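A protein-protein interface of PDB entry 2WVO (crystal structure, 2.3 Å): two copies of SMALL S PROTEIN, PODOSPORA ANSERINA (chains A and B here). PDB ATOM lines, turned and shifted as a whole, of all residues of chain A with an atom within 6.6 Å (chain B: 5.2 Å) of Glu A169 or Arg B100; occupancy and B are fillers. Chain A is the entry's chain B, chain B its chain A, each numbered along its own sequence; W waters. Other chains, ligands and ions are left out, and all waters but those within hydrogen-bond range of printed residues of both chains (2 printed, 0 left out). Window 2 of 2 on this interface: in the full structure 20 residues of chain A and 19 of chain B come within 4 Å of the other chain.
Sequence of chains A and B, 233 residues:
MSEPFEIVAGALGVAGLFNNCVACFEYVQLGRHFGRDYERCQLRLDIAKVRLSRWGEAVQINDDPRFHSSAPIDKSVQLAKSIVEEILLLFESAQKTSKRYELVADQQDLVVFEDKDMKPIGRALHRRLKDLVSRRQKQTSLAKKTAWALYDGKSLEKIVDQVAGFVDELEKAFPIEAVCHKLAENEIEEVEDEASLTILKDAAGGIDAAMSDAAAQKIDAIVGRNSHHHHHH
OE1 of Glu A86 sits at hydrogen-bond distance from OG1 of Thr B97 (3.3 Å).
The guanidinium group (NH1) of Arg B100 is in hydrogen-bond range of the side-chain hydroxyl (OG) of Ser A82 (3.2 Å).
The side-chain carboxylate (OE2) of Glu A86 is in salt-bridge range of the guanidinium group (NH1) of Arg B100 (2.4 Å).
NE of Arg B100 lies within salt-bridge range of OE1 of Glu A169 (3.7 Å).
NH2 of Arg B100 is in hydrogen-bond range of OG1 of Thr B97 (3.1 Å).
NE2 of Gln A78 touches CD2 of Leu B103, at 3.6 Å.
O of Arg B100 touches CD2 of Leu A79, at 3.7 Å.
CD2 of Leu A79 touches CD2 of Leu B103, 3.8 Å away.
O of Ser A82 touches NZ of Lys B96 (3.9 Å).
CD of Arg B100 touches CG1 of Ile A83, 3.8 Å away.
OE2 of Glu A86 touches CB of Lys B96, at 3.5 Å.
Phe A166 touches Arg B100.
Of the printed residues of chain B, Gln A78 touches Leu B103.
Of the printed residues of chain B, Ile A83 touches Arg B100 (3.8 Å).
Of the printed residues of chain B, Glu A86 touches Lys B96 (3.5 Å), Thr B97 (3.3 Å) and Arg B100 (2.4 Å).
Glu A169 touches one residue of chain B.
Of chain A, only Leu A79, Ser A82, Ile A83, Glu A86, Phe A166 and Glu A169 come within 4 Å of Arg B100.
Printed residues of chain A within 4 Å of Leu B103: Gln A78 (3.6 Å) and Leu A79 (3.8 Å).
The nearest printed residue of chain B that does not touch Glu A169 is Thr B97 (6.1 Å).
Hydrophobic or aromatic side chains of chain B that line the printed part of chain A: Leu B103.
Along chain B the printed residues that touch a printed residue of chain A span positions 96 to 103.
Hydrophobic or aromatic side chains of chain A within 4 Å of the printed part of chain B: Leu A79, Ile A83 and Phe A166.
Among the printed residues, Asp or Glu carboxylates within 4 Å of a Lys or Arg side-chain nitrogen of the other chain: Glu A86 with Arg B100 and Glu A169 with Arg B100.
No position is printed for both chains.
Of the 11 pairs that touch across the chains among the printed residues, none has its exchanged pair printed and touching as well.
Water W1 bridges the side-chain hydroxyl of Ser A82 and the side-chain amino group of Lys B96.
Water W2 lies within hydrogen-bond range of OE1 of Glu A86 (2.9 Å) and OG1 of Thr B97 (3.2 Å).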
ATOM      1  N   ARG A  51      -0.811  19.046 -14.780  1.00  0.00           N
ATOM      2  CA  ARG A  51      -1.464  17.820 -15.170  1.00  0.00           C
ATOM      3  C   ARG A  51      -2.779  18.126 -15.908  1.00  0.00           C
ATOM      4  O   ARG A  51      -3.007  17.660 -17.037  1.00  0.00           O
ATOM      5  CB  ARG A  51      -1.713  17.053 -13.873  1.00  0.00           C
ATOM      6  CG  ARG A  51      -2.119  15.631 -13.989  1.00  0.00           C
ATOM      7  CD  ARG A  51      -0.992  14.728 -14.400  1.00  0.00           C
ATOM      8  NE  ARG A  51      -1.599  13.621 -15.120  1.00  0.00           N
ATOM      9  CZ  ARG A  51      -2.164  12.573 -14.538  1.00  0.00           C
ATOM     10  NH1 ARG A  51      -2.156  12.455 -13.219  1.00  0.00           N
ATOM     11  NH2 ARG A  51      -2.716  11.632 -15.285  1.00  0.00           N
ATOM     12  N   TRP A  55      -3.712  17.891 -20.256  1.00  0.00           N
ATOM     13  CA  TRP A  55      -4.883  17.274 -20.881  1.00  0.00           C
ATOM     14  C   TRP A  55      -5.613  18.219 -21.852  1.00  0.00           C
ATOM     15  O   TRP A  55      -6.005  17.809 -22.954  1.00  0.00           O
ATOM     16  CB  TRP A  55      -5.870  16.735 -19.832  1.00  0.00           C
ATOM     17  CG  TRP A  55      -7.115  16.146 -20.472  1.00  0.00           C
ATOM     18  CD1 TRP A  55      -7.261  14.884 -20.979  1.00  0.00           C
ATOM     19  CD2 TRP A  55      -8.373  16.814 -20.690  1.00  0.00           C
ATOM     20  NE1 TRP A  55      -8.528  14.723 -21.494  1.00  0.00           N
ATOM     21  CE2 TRP A  55      -9.232  15.888 -21.325  1.00  0.00           C
ATOM     22  CE3 TRP A  55      -8.850  18.102 -20.410  1.00  0.00           C
ATOM     23  CZ2 TRP A  55     -10.546  16.209 -21.685  1.00  0.00           C
ATOM     24  CZ3 TRP A  55     -10.156  18.424 -20.771  1.00  0.00           C
ATOM     25  CH2 TRP A  55     -10.987  17.479 -21.404  1.00  0.00           C
ATOM     26  N   GLN A  78     -19.281  13.999 -22.522  1.00  0.00           N
ATOM     27  CA  GLN A  78     -20.155  13.901 -21.345  1.00  0.00           C
ATOM     28  C   GLN A  78     -19.408  13.419 -20.105  1.00  0.00           C
ATOM     29  O   GLN A  78     -19.685  13.880 -18.999  1.00  0.00           O
ATOM     30  CB  GLN A  78     -21.322  12.944 -21.605  1.00  0.00           C
ATOM     31  CG  GLN A  78     -22.372  13.467 -22.578  1.00  0.00           C
ATOM     32  CD  GLN A  78     -23.431  12.430 -22.906  1.00  0.00           C
ATOM     33  OE1 GLN A  78     -24.005  12.438 -23.993  1.00  0.00           O
ATOM     34  NE2 GLN A  78     -23.693  11.538 -21.976  1.00  0.00           N
ATOM     35  N   LEU A  79     -18.488  12.478 -20.290  1.00  0.00           N
ATOM     36  CA  LEU A  79     -17.659  12.010 -19.185  1.00  0.00           C
ATOM     37  C   LEU A  79     -16.756  13.126 -18.669  1.00  0.00           C
ATOM     38  O   LEU A  79     -16.677  13.354 -17.472  1.00  0.00           O
ATOM     39  CB  LEU A  79     -16.832  10.784 -19.598  1.00  0.00           C
ATOM     40  CG  LEU A  79     -17.575   9.454 -19.688  1.00  0.00           C
ATOM     41  CD1 LEU A  79     -16.639   8.341 -20.173  1.00  0.00           C
ATOM     42  CD2 LEU A  79     -18.235   9.058 -18.335  1.00  0.00           C
ATOM     43  N   ALA A  80     -16.104  13.817 -19.606  1.00  0.00           N
ATOM     44  CA  ALA A  80     -15.232  14.955 -19.340  1.00  0.00           C
ATOM     45  C   ALA A  80     -15.925  16.077 -18.576  1.00  0.00           C
ATOM     46  O   ALA A  80     -15.339  16.669 -17.672  1.00  0.00           O
ATOM     47  CB  ALA A  80     -14.631  15.504 -20.676  1.00  0.00           C
ATOM     48  N   SER A  82     -18.642  15.833 -16.647  1.00  0.00           N
ATOM     49  CA  SER A  82     -18.911  15.350 -15.299  1.00  0.00           C
ATOM     50  C   SER A  82     -17.689  15.467 -14.369  1.00  0.00           C
ATOM     51  O   SER A  82     -17.792  15.968 -13.260  1.00  0.00           O
ATOM     52  CB  SER A  82     -19.421  13.908 -15.370  1.00  0.00           C
ATOM     53  OG  SER A  82     -19.878  13.473 -14.110  1.00  0.00           O
ATOM     54  N   ILE A  83     -16.531  15.035 -14.861  1.00  0.00           N
ATOM     55  CA  ILE A  83     -15.259  15.068 -14.119  1.00  0.00           C
ATOM     56  C   ILE A  83     -14.873  16.500 -13.757  1.00  0.00           C
ATOM     57  O   ILE A  83     -14.530  16.816 -12.617  1.00  0.00           O
ATOM     58  CB  ILE A  83     -14.130  14.397 -14.976  1.00  0.00           C
ATOM     59  CG1 ILE A  83     -14.328  12.874 -15.005  1.00  0.00           C
ATOM     60  CG2 ILE A  83     -12.746  14.745 -14.443  1.00  0.00           C
ATOM     61  CD1 ILE A  83     -13.807  12.160 -16.271  1.00  0.00           C
ATOM     62  N   VAL A  84     -14.950  17.366 -14.753  1.00  0.00           N
ATOM     63  CA  VAL A  84     -14.592  18.767 -14.623  1.00  0.00           C
ATOM     64  C   VAL A  84     -15.549  19.498 -13.635  1.00  0.00           C
ATOM     65  O   VAL A  84     -15.128  20.306 -12.805  1.00  0.00           O
ATOM     66  CB  VAL A  84     -14.423  19.330 -16.093  1.00  0.00           C
ATOM     67  CG1 VAL A  84     -15.502  20.312 -16.550  1.00  0.00           C
ATOM     68  CG2 VAL A  84     -12.988  19.725 -16.392  1.00  0.00           C
ATOM     69  N   GLU A  86     -16.958  17.852 -11.163  1.00  0.00           N
ATOM     70  CA  GLU A  86     -16.546  17.244  -9.901  1.00  0.00           C
ATOM     71  C   GLU A  86     -15.265  17.880  -9.313  1.00  0.00           C
ATOM     72  O   GLU A  86     -15.138  18.002  -8.095  1.00  0.00           O
ATOM     73  CB  GLU A  86     -16.477  15.684  -9.995  1.00  0.00           C
ATOM     74  CG  GLU A  86     -17.109  15.021  -8.700  1.00  0.00           C
ATOM     75  CD  GLU A  86     -17.329  13.524  -8.741  1.00  0.00           C
ATOM     76  OE1 GLU A  86     -17.227  12.886  -7.670  1.00  0.00           O
ATOM     77  OE2 GLU A  86     -17.625  12.955  -9.804  1.00  0.00           O
ATOM     78  N   ALA A 164      -5.429  14.427  -9.686  1.00  0.00           N
ATOM     79  CA  ALA A 164      -4.605  13.447 -10.395  1.00  0.00           C
ATOM     80  C   ALA A 164      -5.425  12.234 -10.860  1.00  0.00           C
ATOM     81  O   ALA A 164      -5.326  11.825 -12.017  1.00  0.00           O
ATOM     82  CB  ALA A 164      -3.419  13.009  -9.525  1.00  0.00           C
ATOM     83  N   GLY A 165      -6.231  11.674  -9.956  1.00  0.00           N
ATOM     84  CA  GLY A 165      -7.180  10.602 -10.277  1.00  0.00           C
ATOM     85  C   GLY A 165      -8.195  10.960 -11.357  1.00  0.00           C
ATOM     86  O   GLY A 165      -8.508  10.127 -12.218  1.00  0.00           O
ATOM     87  N   PHE A 166      -8.694  12.198 -11.325  1.00  0.00           N
ATOM     88  CA  PHE A 166      -9.633  12.712 -12.343  1.00  0.00           C
ATOM     89  C   PHE A 166      -8.980  12.961 -13.706  1.00  0.00           C
ATOM     90  O   PHE A 166      -9.598  12.714 -14.745  1.00  0.00           O
ATOM     91  CB  PHE A 166     -10.319  14.004 -11.876  1.00  0.00           C
ATOM     92  CG  PHE A 166     -11.415  13.799 -10.863  1.00  0.00           C
ATOM     93  CD1 PHE A 166     -11.500  14.618  -9.735  1.00  0.00           C
ATOM     94  CD2 PHE A 166     -12.382  12.812 -11.041  1.00  0.00           C
ATOM     95  CE1 PHE A 166     -12.519  14.444  -8.797  1.00  0.00           C
ATOM     96  CE2 PHE A 166     -13.400  12.634 -10.092  1.00  0.00           C
ATOM     97  CZ  PHE A 166     -13.460  13.454  -8.975  1.00  0.00           C
ATOM     98  N   VAL A 167      -7.742  13.448 -13.718  1.00  0.00           N
ATOM     99  CA  VAL A 167      -7.017  13.624 -14.981  1.00  0.00           C
ATOM    100  C   VAL A 167      -6.688  12.266 -15.622  1.00  0.00           C
ATOM    101  O   VAL A 167      -6.624  12.157 -16.855  1.00  0.00           O
ATOM    102  CB  VAL A 167      -5.763  14.546 -14.855  1.00  0.00           C
ATOM    103  CG1 VAL A 167      -5.053  14.696 -16.209  1.00  0.00           C
ATOM    104  CG2 VAL A 167      -6.160  15.938 -14.347  1.00  0.00           C
ATOM    105  N   ASP A 168      -6.511  11.242 -14.786  1.00  0.00           N
ATOM    106  CA  ASP A 168      -6.399   9.851 -15.240  1.00  0.00           C
ATOM    107  C   ASP A 168      -7.654   9.434 -16.017  1.00  0.00           C
ATOM    108  O   ASP A 168      -7.562   8.955 -17.147  1.00  0.00           O
ATOM    109  CB  ASP A 168      -6.164   8.903 -14.046  1.00  0.00           C
ATOM    110  CG  ASP A 168      -4.722   8.921 -13.541  1.00  0.00           C
ATOM    111  OD1 ASP A 168      -4.470   8.435 -12.407  1.00  0.00           O
ATOM    112  OD2 ASP A 168      -3.837   9.405 -14.278  1.00  0.00           O
ATOM    113  N   GLU A 169      -8.817   9.631 -15.399  1.00  0.00           N
ATOM    114  CA  GLU A 169     -10.119   9.383 -16.020  1.00  0.00           C
ATOM    115  C   GLU A 169     -10.322  10.199 -17.299  1.00  0.00           C
ATOM    116  O   GLU A 169     -10.938   9.727 -18.257  1.00  0.00           O
ATOM    117  CB  GLU A 169     -11.253   9.721 -15.047  1.00  0.00           C
ATOM    118  CG  GLU A 169     -11.399   8.804 -13.862  1.00  0.00           C
ATOM    119  CD  GLU A 169     -12.781   8.906 -13.233  1.00  0.00           C
ATOM    120  OE1 GLU A 169     -13.764   8.435 -13.867  1.00  0.00           O
ATOM    121  OE2 GLU A 169     -12.886   9.446 -12.103  1.00  0.00           O
ATOM    122  N   LEU A 170      -9.813  11.430 -17.292  1.00  0.00           N
ATOM    123  CA  LEU A 170      -9.855  12.321 -18.452  1.00  0.00           C
ATOM    124  C   LEU A 170      -9.023  11.763 -19.606  1.00  0.00           C
ATOM    125  O   LEU A 170      -9.469  11.755 -20.757  1.00  0.00           O
ATOM    126  CB  LEU A 170      -9.366  13.724 -18.058  1.00  0.00           C
ATOM    127  CG  LEU A 170     -10.255  14.983 -17.987  1.00  0.00           C
ATOM    128  CD1 LEU A 170     -11.769  14.742 -18.014  1.00  0.00           C
ATOM    129  CD2 LEU A 170      -9.843  15.915 -16.857  1.00  0.00           C
ATOM    130  N   GLU A 171      -7.818  11.297 -19.295  1.00  0.00           N
ATOM    131  CA  GLU A 171      -6.910  10.752 -20.302  1.00  0.00           C
ATOM    132  C   GLU A 171      -7.414   9.432 -20.892  1.00  0.00           C
ATOM    133  O   GLU A 171      -7.212   9.170 -22.077  1.00  0.00           O
ATOM    134  CB  GLU A 171      -5.491  10.602 -19.736  1.00  0.00           C
ATOM    135  CG  GLU A 171      -4.770  11.939 -19.514  1.00  0.00           C
ATOM    136  CD  GLU A 171      -3.421  11.810 -18.805  1.00  0.00           C
ATOM    137  OE1 GLU A 171      -2.923  12.834 -18.284  1.00  0.00           O
ATOM    138  OE2 GLU A 171      -2.853  10.695 -18.770  1.00  0.00           O
ATOM    139  N   LYS A 172      -8.080   8.615 -20.073  1.00  0.00           N
ATOM    140  CA  LYS A 172      -8.670   7.350 -20.538  1.00  0.00           C
ATOM    141  C   LYS A 172      -9.807   7.558 -21.548  1.00  0.00           C
ATOM    142  O   LYS A 172      -9.997   6.737 -22.448  1.00  0.00           O
ATOM    143  CB  LYS A 172      -9.142   6.494 -19.348  1.00  0.00           C
ATOM    144  CG  LYS A 172     -10.125   5.371 -19.713  1.00  0.00           C
ATOM    145  CD  LYS A 172      -9.939   4.106 -18.879  1.00  0.00           C
ATOM    146  CE  LYS A 172     -10.572   4.219 -17.497  1.00  0.00           C
ATOM    147  NZ  LYS A 172     -10.575   2.890 -16.804  1.00  0.00           N
ATOM    148  N   ALA A 173     -10.543   8.659 -21.399  1.00  0.00           N
ATOM    149  CA  ALA A 173     -11.712   8.942 -22.226  1.00  0.00           C
ATOM    150  C   ALA A 173     -11.348   9.446 -23.623  1.00  0.00           C
ATOM    151  O   ALA A 173     -12.215   9.562 -24.487  1.00  0.00           O
ATOM    152  CB  ALA A 173     -12.622   9.945 -21.519  1.00  0.00           C
ATOM    153  N   PHE A 174     -10.069   9.748 -23.834  1.00  0.00           N
ATOM    154  CA  PHE A 174      -9.597  10.348 -25.081  1.00  0.00           C
ATOM    155  C   PHE A 174      -8.341   9.664 -25.646  1.00  0.00           C
ATOM    156  O   PHE A 174      -7.488   9.198 -24.886  1.00  0.00           O
ATOM    157  CB  PHE A 174      -9.402  11.862 -24.896  1.00  0.00           C
ATOM    158  CG  PHE A 174     -10.695  12.606 -24.703  1.00  0.00           C
ATOM    159  CD1 PHE A 174     -11.255  12.739 -23.433  1.00  0.00           C
ATOM    160  CD2 PHE A 174     -11.382  13.125 -25.797  1.00  0.00           C
ATOM    161  CE1 PHE A 174     -12.461  13.388 -23.253  1.00  0.00           C
ATOM    162  CE2 PHE A 174     -12.588  13.786 -25.631  1.00  0.00           C
ATOM    163  CZ  PHE A 174     -13.132  13.917 -24.353  1.00  0.00           C
ATOM    164  N   GLN B  95     -23.415  10.651  -6.827  1.00  0.00           N
ATOM    165  CA  GLN B  95     -24.338  10.469  -7.956  1.00  0.00           C
ATOM    166  C   GLN B  95     -23.664  10.690  -9.318  1.00  0.00           C
ATOM    167  O   GLN B  95     -23.935   9.978 -10.262  1.00  0.00           O
ATOM    168  CB  GLN B  95     -25.573  11.365  -7.809  1.00  0.00           C
ATOM    169  CG  GLN B  95     -26.551  10.836  -6.779  1.00  0.00           C
ATOM    170  CD  GLN B  95     -27.672  11.812  -6.407  1.00  0.00           C
ATOM    171  OE1 GLN B  95     -27.875  12.099  -5.234  1.00  0.00           O
ATOM    172  NE2 GLN B  95     -28.413  12.286  -7.393  1.00  0.00           N
ATOM    173  N   LYS B  96     -22.775  11.674  -9.391  1.00  0.00           N
ATOM    174  CA  LYS B  96     -21.982  11.954 -10.587  1.00  0.00           C
ATOM    175  C   LYS B  96     -21.081  10.777 -10.961  1.00  0.00           C
ATOM    176  O   LYS B  96     -21.038  10.370 -12.113  1.00  0.00           O
ATOM    177  CB  LYS B  96     -21.117  13.190 -10.350  1.00  0.00           C
ATOM    178  CG  LYS B  96     -21.892  14.491 -10.250  1.00  0.00           C
ATOM    179  CD  LYS B  96     -20.914  15.633 -10.157  1.00  0.00           C
ATOM    180  CE  LYS B  96     -21.421  16.843 -10.895  1.00  0.00           C
ATOM    181  NZ  LYS B  96     -21.474  16.680 -12.350  1.00  0.00           N
ATOM    182  N   THR B  97     -20.357  10.251  -9.976  1.00  0.00           N
ATOM    183  CA  THR B  97     -19.472   9.111 -10.169  1.00  0.00           C
ATOM    184  C   THR B  97     -20.258   7.930 -10.702  1.00  0.00           C
ATOM    185  O   THR B  97     -19.842   7.301 -11.670  1.00  0.00           O
ATOM    186  CB  THR B  97     -18.755   8.713  -8.859  1.00  0.00           C
ATOM    187  OG1 THR B  97     -17.812   9.722  -8.522  1.00  0.00           O
ATOM    188  CG2 THR B  97     -18.016   7.363  -8.996  1.00  0.00           C
ATOM    189  N   SER B  98     -21.387   7.657 -10.057  1.00  0.00           N
ATOM    190  CA  SER B  98     -22.314   6.599 -10.446  1.00  0.00           C
ATOM    191  C   SER B  98     -22.812   6.767 -11.886  1.00  0.00           C
ATOM    192  O   SER B  98     -22.838   5.803 -12.648  1.00  0.00           O
ATOM    193  CB  SER B  98     -23.479   6.536  -9.443  1.00  0.00           C
ATOM    194  OG  SER B  98     -24.587   5.806  -9.955  1.00  0.00           O
ATOM    195  N   LYS B  99     -23.198   7.983 -12.255  1.00  0.00           N
ATOM    196  CA  LYS B  99     -23.571   8.296 -13.633  1.00  0.00           C
ATOM    197  C   LYS B  99     -22.473   8.031 -14.650  1.00  0.00           C
ATOM    198  O   LYS B  99     -22.752   7.541 -15.748  1.00  0.00           O
ATOM    199  CB  LYS B  99     -24.043   9.742 -13.748  1.00  0.00           C
ATOM    200  CG  LYS B  99     -25.535   9.827 -13.804  1.00  0.00           C
ATOM    201  CD  LYS B  99     -26.078  10.742 -12.753  1.00  0.00           C
ATOM    202  CE  LYS B  99     -26.370  12.118 -13.293  1.00  0.00           C
ATOM    203  NZ  LYS B  99     -27.359  12.748 -12.385  1.00  0.00           N
ATOM    204  N   ARG B 100     -21.230   8.354 -14.295  1.00  0.00           N
ATOM    205  CA  ARG B 100     -20.097   8.063 -15.174  1.00  0.00           C
ATOM    206  C   ARG B 100     -19.922   6.557 -15.381  1.00  0.00           C
ATOM    207  O   ARG B 100     -19.534   6.112 -16.471  1.00  0.00           O
ATOM    208  CB  ARG B 100     -18.815   8.706 -14.649  1.00  0.00           C
ATOM    209  CG  ARG B 100     -18.840  10.216 -14.760  1.00  0.00           C
ATOM    210  CD  ARG B 100     -17.464  10.838 -14.583  1.00  0.00           C
ATOM    211  NE  ARG B 100     -16.812  10.473 -13.324  1.00  0.00           N
ATOM    212  CZ  ARG B 100     -16.984  11.107 -12.171  1.00  0.00           C
ATOM    213  NH1 ARG B 100     -17.822  12.148 -12.081  1.00  0.00           N
ATOM    214  NH2 ARG B 100     -16.315  10.699 -11.099  1.00  0.00           N
ATOM    215  N   TYR B 101     -20.230   5.781 -14.339  1.00  0.00           N
ATOM    216  CA  TYR B 101     -20.152   4.323 -14.403  1.00  0.00           C
ATOM    217  C   TYR B 101     -21.222   3.743 -15.332  1.00  0.00           C
ATOM    218  O   TYR B 101     -20.918   2.899 -16.169  1.00  0.00           O
ATOM    219  CB  TYR B 101     -20.255   3.709 -13.003  1.00  0.00           C
ATOM    220  CG  TYR B 101     -19.983   2.222 -12.958  1.00  0.00           C
ATOM    221  CD1 TYR B 101     -18.684   1.744 -12.843  1.00  0.00           C
ATOM    222  CD2 TYR B 101     -21.026   1.291 -13.041  1.00  0.00           C
ATOM    223  CE1 TYR B 101     -18.417   0.372 -12.813  1.00  0.00           C
ATOM    224  CE2 TYR B 101     -20.775  -0.082 -12.991  1.00  0.00           C
ATOM    225  CZ  TYR B 101     -19.462  -0.534 -12.877  1.00  0.00           C
ATOM    226  OH  TYR B 101     -19.179  -1.893 -12.846  1.00  0.00           O
ATOM    227  N   GLU B 102     -22.462   4.204 -15.179  1.00  0.00           N
ATOM    228  CA  GLU B 102     -23.584   3.748 -16.001  1.00  0.00           C
ATOM    229  C   GLU B 102     -23.423   4.074 -17.474  1.00  0.00           C
ATOM    230  O   GLU B 102     -23.988   3.391 -18.320  1.00  0.00           O
ATOM    231  CB  GLU B 102     -24.882   4.396 -15.554  1.00  0.00           C
ATOM    232  CG  GLU B 102     -25.395   3.966 -14.219  1.00  0.00           C
ATOM    233  CD  GLU B 102     -26.678   4.688 -13.878  1.00  0.00           C
ATOM    234  OE1 GLU B 102     -27.552   4.064 -13.238  1.00  0.00           O
ATOM    235  OE2 GLU B 102     -26.814   5.879 -14.260  1.00  0.00           O
ATOM    236  N   LEU B 103     -22.685   5.141 -17.766  1.00  0.00           N
ATOM    237  CA  LEU B 103     -22.446   5.582 -19.133  1.00  0.00           C
ATOM    238  C   LEU B 103     -21.544   4.592 -19.895  1.00  0.00           C
ATOM    239  O   LEU B 103     -21.681   4.417 -21.108  1.00  0.00           O
ATOM    240  CB  LEU B 103     -21.821   6.977 -19.116  1.00  0.00           C
ATOM    241  CG  LEU B 103     -22.269   8.011 -20.153  1.00  0.00           C
ATOM    242  CD1 LEU B 103     -23.796   8.048 -20.354  1.00  0.00           C
ATOM    243  CD2 LEU B 103     -21.741   9.383 -19.776  1.00  0.00           C
ATOM    244  N   VAL B 104     -20.649   3.929 -19.161  1.00  0.00           N
ATOM    245  CA  VAL B 104     -19.572   3.148 -19.765  1.00  0.00           C
ATOM    246  C   VAL B 104     -19.726   1.624 -19.564  1.00  0.00           C
ATOM    247  O   VAL B 104     -19.192   0.837 -20.339  1.00  0.00           O
ATOM    248  CB  VAL B 104     -18.176   3.675 -19.279  1.00  0.00           C
ATOM    249  CG1 VAL B 104     -17.796   3.089 -17.918  1.00  0.00           C
ATOM    250  CG2 VAL B 104     -17.092   3.412 -20.311  1.00  0.00           C
HETATM  251  O   HOH W   1     -22.512  13.718 -13.751  1.00  0.00           O
HETATM  252  O   HOH W   2     -17.729  10.926  -5.555  1.00  0.00           O
